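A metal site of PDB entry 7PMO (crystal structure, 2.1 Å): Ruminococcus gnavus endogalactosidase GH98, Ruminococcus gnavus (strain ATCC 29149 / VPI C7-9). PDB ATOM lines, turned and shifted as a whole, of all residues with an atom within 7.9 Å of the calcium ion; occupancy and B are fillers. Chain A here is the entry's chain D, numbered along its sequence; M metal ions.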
ATOM      1  N   ALA A  27      19.294   7.405 -14.064  1.00  0.00           N
ATOM      2  CA  ALA A  27      19.849   8.384 -15.042  1.00  0.00           C
ATOM      3  C   ALA A  27      21.286   8.001 -15.434  1.00  0.00           C
ATOM      4  O   ALA A  27      21.661   8.351 -16.574  1.00  0.00           O
ATOM      5  CB  ALA A  27      19.785   9.792 -14.484  1.00  0.00           C
ATOM      6  N   ASP A  28      22.024   7.313 -14.557  1.00  0.00           N
ATOM      7  CA  ASP A  28      23.469   6.962 -14.742  1.00  0.00           C
ATOM      8  C   ASP A  28      23.663   5.990 -15.914  1.00  0.00           C
ATOM      9  O   ASP A  28      24.759   5.981 -16.486  1.00  0.00           O
ATOM     10  CB  ASP A  28      24.082   6.326 -13.484  1.00  0.00           C
ATOM     11  CG  ASP A  28      24.349   7.297 -12.337  1.00  0.00           C
ATOM     12  OD1 ASP A  28      24.703   8.463 -12.603  1.00  0.00           O
ATOM     13  OD2 ASP A  28      24.185   6.882 -11.176  1.00  0.00           O
ATOM     14  N   LEU A  29      22.654   5.186 -16.246  1.00  0.00           N
ATOM     15  CA  LEU A  29      22.764   4.097 -17.253  1.00  0.00           C
ATOM     16  C   LEU A  29      22.924   4.681 -18.657  1.00  0.00           C
ATOM     17  O   LEU A  29      23.497   3.985 -19.500  1.00  0.00           O
ATOM     18  CB  LEU A  29      21.532   3.199 -17.153  1.00  0.00           C
ATOM     19  CG  LEU A  29      21.430   2.403 -15.854  1.00  0.00           C
ATOM     20  CD1 LEU A  29      20.168   1.560 -15.842  1.00  0.00           C
ATOM     21  CD2 LEU A  29      22.667   1.547 -15.644  1.00  0.00           C
ATOM     22  N   LEU A  30      22.458   5.909 -18.878  1.00  0.00           N
ATOM     23  CA  LEU A  30      22.421   6.595 -20.209  1.00  0.00           C
ATOM     24  C   LEU A  30      23.836   6.885 -20.738  1.00  0.00           C
ATOM     25  O   LEU A  30      24.019   6.908 -21.972  1.00  0.00           O
ATOM     26  CB  LEU A  30      21.617   7.887 -20.044  1.00  0.00           C
ATOM     27  CG  LEU A  30      21.283   8.614 -21.340  1.00  0.00           C
ATOM     28  CD1 LEU A  30      20.415   7.742 -22.246  1.00  0.00           C
ATOM     29  CD2 LEU A  30      20.587   9.939 -21.062  1.00  0.00           C
ATOM     30  N   THR A  31      24.806   7.128 -19.850  1.00  0.00           N
ATOM     31  CA  THR A  31      26.149   7.660 -20.183  1.00  0.00           C
ATOM     32  C   THR A  31      27.234   6.819 -19.488  1.00  0.00           C
ATOM     33  O   THR A  31      28.300   7.367 -19.189  1.00  0.00           O
ATOM     34  CB  THR A  31      26.230   9.146 -19.790  1.00  0.00           C
ATOM     35  OG1 THR A  31      26.163   9.289 -18.373  1.00  0.00           O
ATOM     36  CG2 THR A  31      25.142   9.986 -20.433  1.00  0.00           C
ATOM     37  N   ASP A  32      26.969   5.529 -19.238  1.00  0.00           N
ATOM     38  CA  ASP A  32      27.893   4.622 -18.510  1.00  0.00           C
ATOM     39  C   ASP A  32      28.776   3.862 -19.509  1.00  0.00           C
ATOM     40  O   ASP A  32      29.605   3.055 -19.053  1.00  0.00           O
ATOM     41  CB  ASP A  32      27.128   3.659 -17.598  1.00  0.00           C
ATOM     42  CG  ASP A  32      26.196   2.701 -18.320  1.00  0.00           C
ATOM     43  OD1 ASP A  32      26.209   2.680 -19.577  1.00  0.00           O
ATOM     44  OD2 ASP A  32      25.447   1.995 -17.616  1.00  0.00           O
ATOM     45  N   GLY A  33      28.562   4.068 -20.812  1.00  0.00           N
ATOM     46  CA  GLY A  33      29.392   3.480 -21.875  1.00  0.00           C
ATOM     47  C   GLY A  33      29.016   2.051 -22.207  1.00  0.00           C
ATOM     48  O   GLY A  33      29.708   1.454 -23.023  1.00  0.00           O
ATOM     49  N   ASP A  34      27.928   1.541 -21.620  1.00  0.00           N
ATOM     50  CA  ASP A  34      27.500   0.120 -21.741  1.00  0.00           C
ATOM     51  C   ASP A  34      26.202   0.040 -22.569  1.00  0.00           C
ATOM     52  O   ASP A  34      25.171   0.565 -22.116  1.00  0.00           O
ATOM     53  CB  ASP A  34      27.326  -0.520 -20.364  1.00  0.00           C
ATOM     54  CG  ASP A  34      27.357  -2.036 -20.350  1.00  0.00           C
ATOM     55  OD1 ASP A  34      27.220  -2.656 -21.437  1.00  0.00           O
ATOM     56  OD2 ASP A  34      27.509  -2.593 -19.253  1.00  0.00           O
ATOM     57  N   LYS A  35      26.252  -0.645 -23.707  1.00  0.00           N
ATOM     58  CA  LYS A  35      25.092  -0.825 -24.617  1.00  0.00           C
ATOM     59  C   LYS A  35      24.549  -2.255 -24.500  1.00  0.00           C
ATOM     60  O   LYS A  35      23.510  -2.497 -25.116  1.00  0.00           O
ATOM     61  CB  LYS A  35      25.501  -0.507 -26.058  1.00  0.00           C
ATOM     62  CG  LYS A  35      25.970   0.927 -26.277  1.00  0.00           C
ATOM     63  CD  LYS A  35      25.881   1.426 -27.693  1.00  0.00           C
ATOM     64  CE  LYS A  35      26.505   0.510 -28.726  1.00  0.00           C
ATOM     65  NZ  LYS A  35      27.053   1.286 -29.868  1.00  0.00           N
ATOM     66  N   TYR A  36      25.206  -3.149 -23.745  1.00  0.00           N
ATOM     67  CA  TYR A  36      24.977  -4.623 -23.820  1.00  0.00           C
ATOM     68  C   TYR A  36      24.577  -5.226 -22.462  1.00  0.00           C
ATOM     69  O   TYR A  36      23.752  -6.151 -22.477  1.00  0.00           O
ATOM     70  CB  TYR A  36      26.189  -5.299 -24.474  1.00  0.00           C
ATOM     71  CG  TYR A  36      26.569  -4.629 -25.771  1.00  0.00           C
ATOM     72  CD1 TYR A  36      25.710  -4.676 -26.862  1.00  0.00           C
ATOM     73  CD2 TYR A  36      27.727  -3.873 -25.891  1.00  0.00           C
ATOM     74  CE1 TYR A  36      26.012  -4.016 -28.036  1.00  0.00           C
ATOM     75  CE2 TYR A  36      28.046  -3.223 -27.068  1.00  0.00           C
ATOM     76  CZ  TYR A  36      27.183  -3.284 -28.142  1.00  0.00           C
ATOM     77  OH  TYR A  36      27.471  -2.630 -29.308  1.00  0.00           O
ATOM     78  N   TYR A  37      25.157  -4.756 -21.349  1.00  0.00           N
ATOM     79  CA  TYR A  37      24.805  -5.143 -19.960  1.00  0.00           C
ATOM     80  C   TYR A  37      25.020  -6.664 -19.739  1.00  0.00           C
ATOM     81  O   TYR A  37      24.184  -7.326 -19.083  1.00  0.00           O
ATOM     82  CB  TYR A  37      23.397  -4.629 -19.623  1.00  0.00           C
ATOM     83  CG  TYR A  37      23.410  -3.132 -19.456  1.00  0.00           C
ATOM     84  CD1 TYR A  37      23.994  -2.553 -18.352  1.00  0.00           C
ATOM     85  CD2 TYR A  37      22.922  -2.299 -20.449  1.00  0.00           C
ATOM     86  CE1 TYR A  37      24.091  -1.180 -18.233  1.00  0.00           C
ATOM     87  CE2 TYR A  37      22.997  -0.922 -20.338  1.00  0.00           C
ATOM     88  CZ  TYR A  37      23.575  -0.356 -19.218  1.00  0.00           C
ATOM     89  OH  TYR A  37      23.645   1.008 -19.090  1.00  0.00           O
ATOM     90  N   GLN A  57      19.065  -3.303 -19.945  1.00  0.00           N
ATOM     91  CA  GLN A  57      18.962  -2.284 -18.876  1.00  0.00           C
ATOM     92  C   GLN A  57      19.038  -0.896 -19.522  1.00  0.00           C
ATOM     93  O   GLN A  57      19.563  -0.777 -20.648  1.00  0.00           O
ATOM     94  CB  GLN A  57      20.097  -2.482 -17.868  1.00  0.00           C
ATOM     95  CG  GLN A  57      20.194  -3.901 -17.325  1.00  0.00           C
ATOM     96  CD  GLN A  57      21.075  -3.974 -16.113  1.00  0.00           C
ATOM     97  OE1 GLN A  57      20.975  -3.141 -15.212  1.00  0.00           O
ATOM     98  NE2 GLN A  57      21.979  -4.948 -16.081  1.00  0.00           N
ATOM     99  N   GLY A  58      18.548   0.133 -18.832  1.00  0.00           N
ATOM    100  CA  GLY A  58      18.581   1.496 -19.382  1.00  0.00           C
ATOM    101  C   GLY A  58      17.907   2.508 -18.487  1.00  0.00           C
ATOM    102  O   GLY A  58      17.108   2.115 -17.628  1.00  0.00           O
ATOM    103  N   THR A  59      18.225   3.785 -18.721  1.00  0.00           N
ATOM    104  CA  THR A  59      17.526   4.944 -18.116  1.00  0.00           C
ATOM    105  C   THR A  59      16.076   4.921 -18.603  1.00  0.00           C
ATOM    106  O   THR A  59      15.866   4.910 -19.834  1.00  0.00           O
ATOM    107  CB  THR A  59      18.269   6.242 -18.460  1.00  0.00           C
ATOM    108  OG1 THR A  59      19.566   6.146 -17.862  1.00  0.00           O
ATOM    109  CG2 THR A  59      17.545   7.474 -17.970  1.00  0.00           C
ATOM    110  N   LYS A  89      20.886   4.387 -28.502  1.00  0.00           N
ATOM    111  CA  LYS A  89      20.303   3.027 -28.375  1.00  0.00           C
ATOM    112  C   LYS A  89      19.212   3.035 -27.303  1.00  0.00           C
ATOM    113  O   LYS A  89      19.479   3.438 -26.166  1.00  0.00           O
ATOM    114  CB  LYS A  89      21.343   1.957 -28.049  1.00  0.00           C
ATOM    115  CG  LYS A  89      20.775   0.558 -28.111  1.00  0.00           C
ATOM    116  CD  LYS A  89      21.761  -0.529 -27.779  1.00  0.00           C
ATOM    117  CE  LYS A  89      21.127  -1.907 -27.813  1.00  0.00           C
ATOM    118  NZ  LYS A  89      22.074  -2.952 -27.375  1.00  0.00           N
ATOM    119  N   PHE A 206      16.125   4.075 -22.424  1.00  0.00           N
ATOM    120  CA  PHE A 206      17.314   4.619 -23.138  1.00  0.00           C
ATOM    121  C   PHE A 206      18.556   3.901 -22.617  1.00  0.00           C
ATOM    122  O   PHE A 206      18.982   4.154 -21.473  1.00  0.00           O
ATOM    123  CB  PHE A 206      17.410   6.130 -22.947  1.00  0.00           C
ATOM    124  CG  PHE A 206      16.305   6.966 -23.539  1.00  0.00           C
ATOM    125  CD1 PHE A 206      16.330   7.334 -24.869  1.00  0.00           C
ATOM    126  CD2 PHE A 206      15.271   7.443 -22.746  1.00  0.00           C
ATOM    127  CE1 PHE A 206      15.332   8.136 -25.409  1.00  0.00           C
ATOM    128  CE2 PHE A 206      14.273   8.245 -23.286  1.00  0.00           C
ATOM    129  CZ  PHE A 206      14.305   8.587 -24.625  1.00  0.00           C
ATOM    130  N   MET A 207      19.138   3.003 -23.415  1.00  0.00           N
ATOM    131  CA  MET A 207      20.254   2.128 -22.960  1.00  0.00           C
ATOM    132  C   MET A 207      21.584   2.894 -23.067  1.00  0.00           C
ATOM    133  O   MET A 207      22.511   2.611 -22.239  1.00  0.00           O
ATOM    134  CB  MET A 207      20.291   0.835 -23.776  1.00  0.00           C
ATOM    135  CG  MET A 207      18.990   0.054 -23.724  1.00  0.00           C
ATOM    136  SD  MET A 207      19.045  -1.533 -24.606  1.00  0.00           S
ATOM    137  CE  MET A 207      20.291  -2.415 -23.653  1.00  0.00           C
ATOM    138  N   GLU A 208      21.703   3.802 -24.032  1.00  0.00           N
ATOM    139  CA  GLU A 208      22.923   4.626 -24.226  1.00  0.00           C
ATOM    140  C   GLU A 208      22.638   5.829 -25.133  1.00  0.00           C
ATOM    141  O   GLU A 208      22.004   5.664 -26.219  1.00  0.00           O
ATOM    142  CB  GLU A 208      24.072   3.807 -24.839  1.00  0.00           C
ATOM    143  CG  GLU A 208      25.436   4.451 -24.680  1.00  0.00           C
ATOM    144  CD  GLU A 208      26.011   4.472 -23.261  1.00  0.00           C
ATOM    145  OE1 GLU A 208      25.406   3.871 -22.349  1.00  0.00           O
ATOM    146  OE2 GLU A 208      27.050   5.124 -23.056  1.00  0.00           O
ATOM    147  N   LEU A 209      23.132   6.990 -24.714  1.00  0.00           N
ATOM    148  CA  LEU A 209      23.311   8.190 -25.562  1.00  0.00           C
ATOM    149  C   LEU A 209      24.811   8.539 -25.595  1.00  0.00           C
ATOM    150  O   LEU A 209      25.301   9.118 -24.627  1.00  0.00           O
ATOM    151  CB  LEU A 209      22.453   9.329 -25.004  1.00  0.00           C
ATOM    152  CG  LEU A 209      22.407  10.589 -25.865  1.00  0.00           C
ATOM    153  CD1 LEU A 209      22.013  10.277 -27.298  1.00  0.00           C
ATOM    154  CD2 LEU A 209      21.470  11.616 -25.256  1.00  0.00           C
HETATM  155 CA    CA M   1      24.331   2.555 -20.976  1.00  0.00          CA
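Within 4 Å of the calcium ion: Leu 29, Asp 32, Asp 34, Tyr 37, Met 207 and Glu 208.
The calcium ion is bound by the side-chain carboxylate of Glu 208 (2.2 Å), the backbone carbonyl oxygen of Met 207 (2.2 Å), the backbone carbonyl oxygen of Leu 29 (2.2 Å), the side-chain carboxylate of Asp 32 (2.3 Å), the backbone carbonyl oxygen of Asp 34 (2.4 Å) and the side-chain hydroxyl of Tyr 37 (2.5 Å).
The backbone NH (N) of Met 207 is in hydrogen-bond range of the backbone carbonyl oxygen (O) of Lys 89.
N of Tyr 36 lies within hydrogen-bond range of OD1 of Asp 34 (3.1 Å).
The backbone NH (N) of Gly 33 sits at hydrogen-bond distance from the side-chain carboxylate (OE2) of Glu 208.
The backbone carbonyl oxygen (O) of Glu 208 sits at hydrogen-bond distance from the backbone NH (N) of Lys 89.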
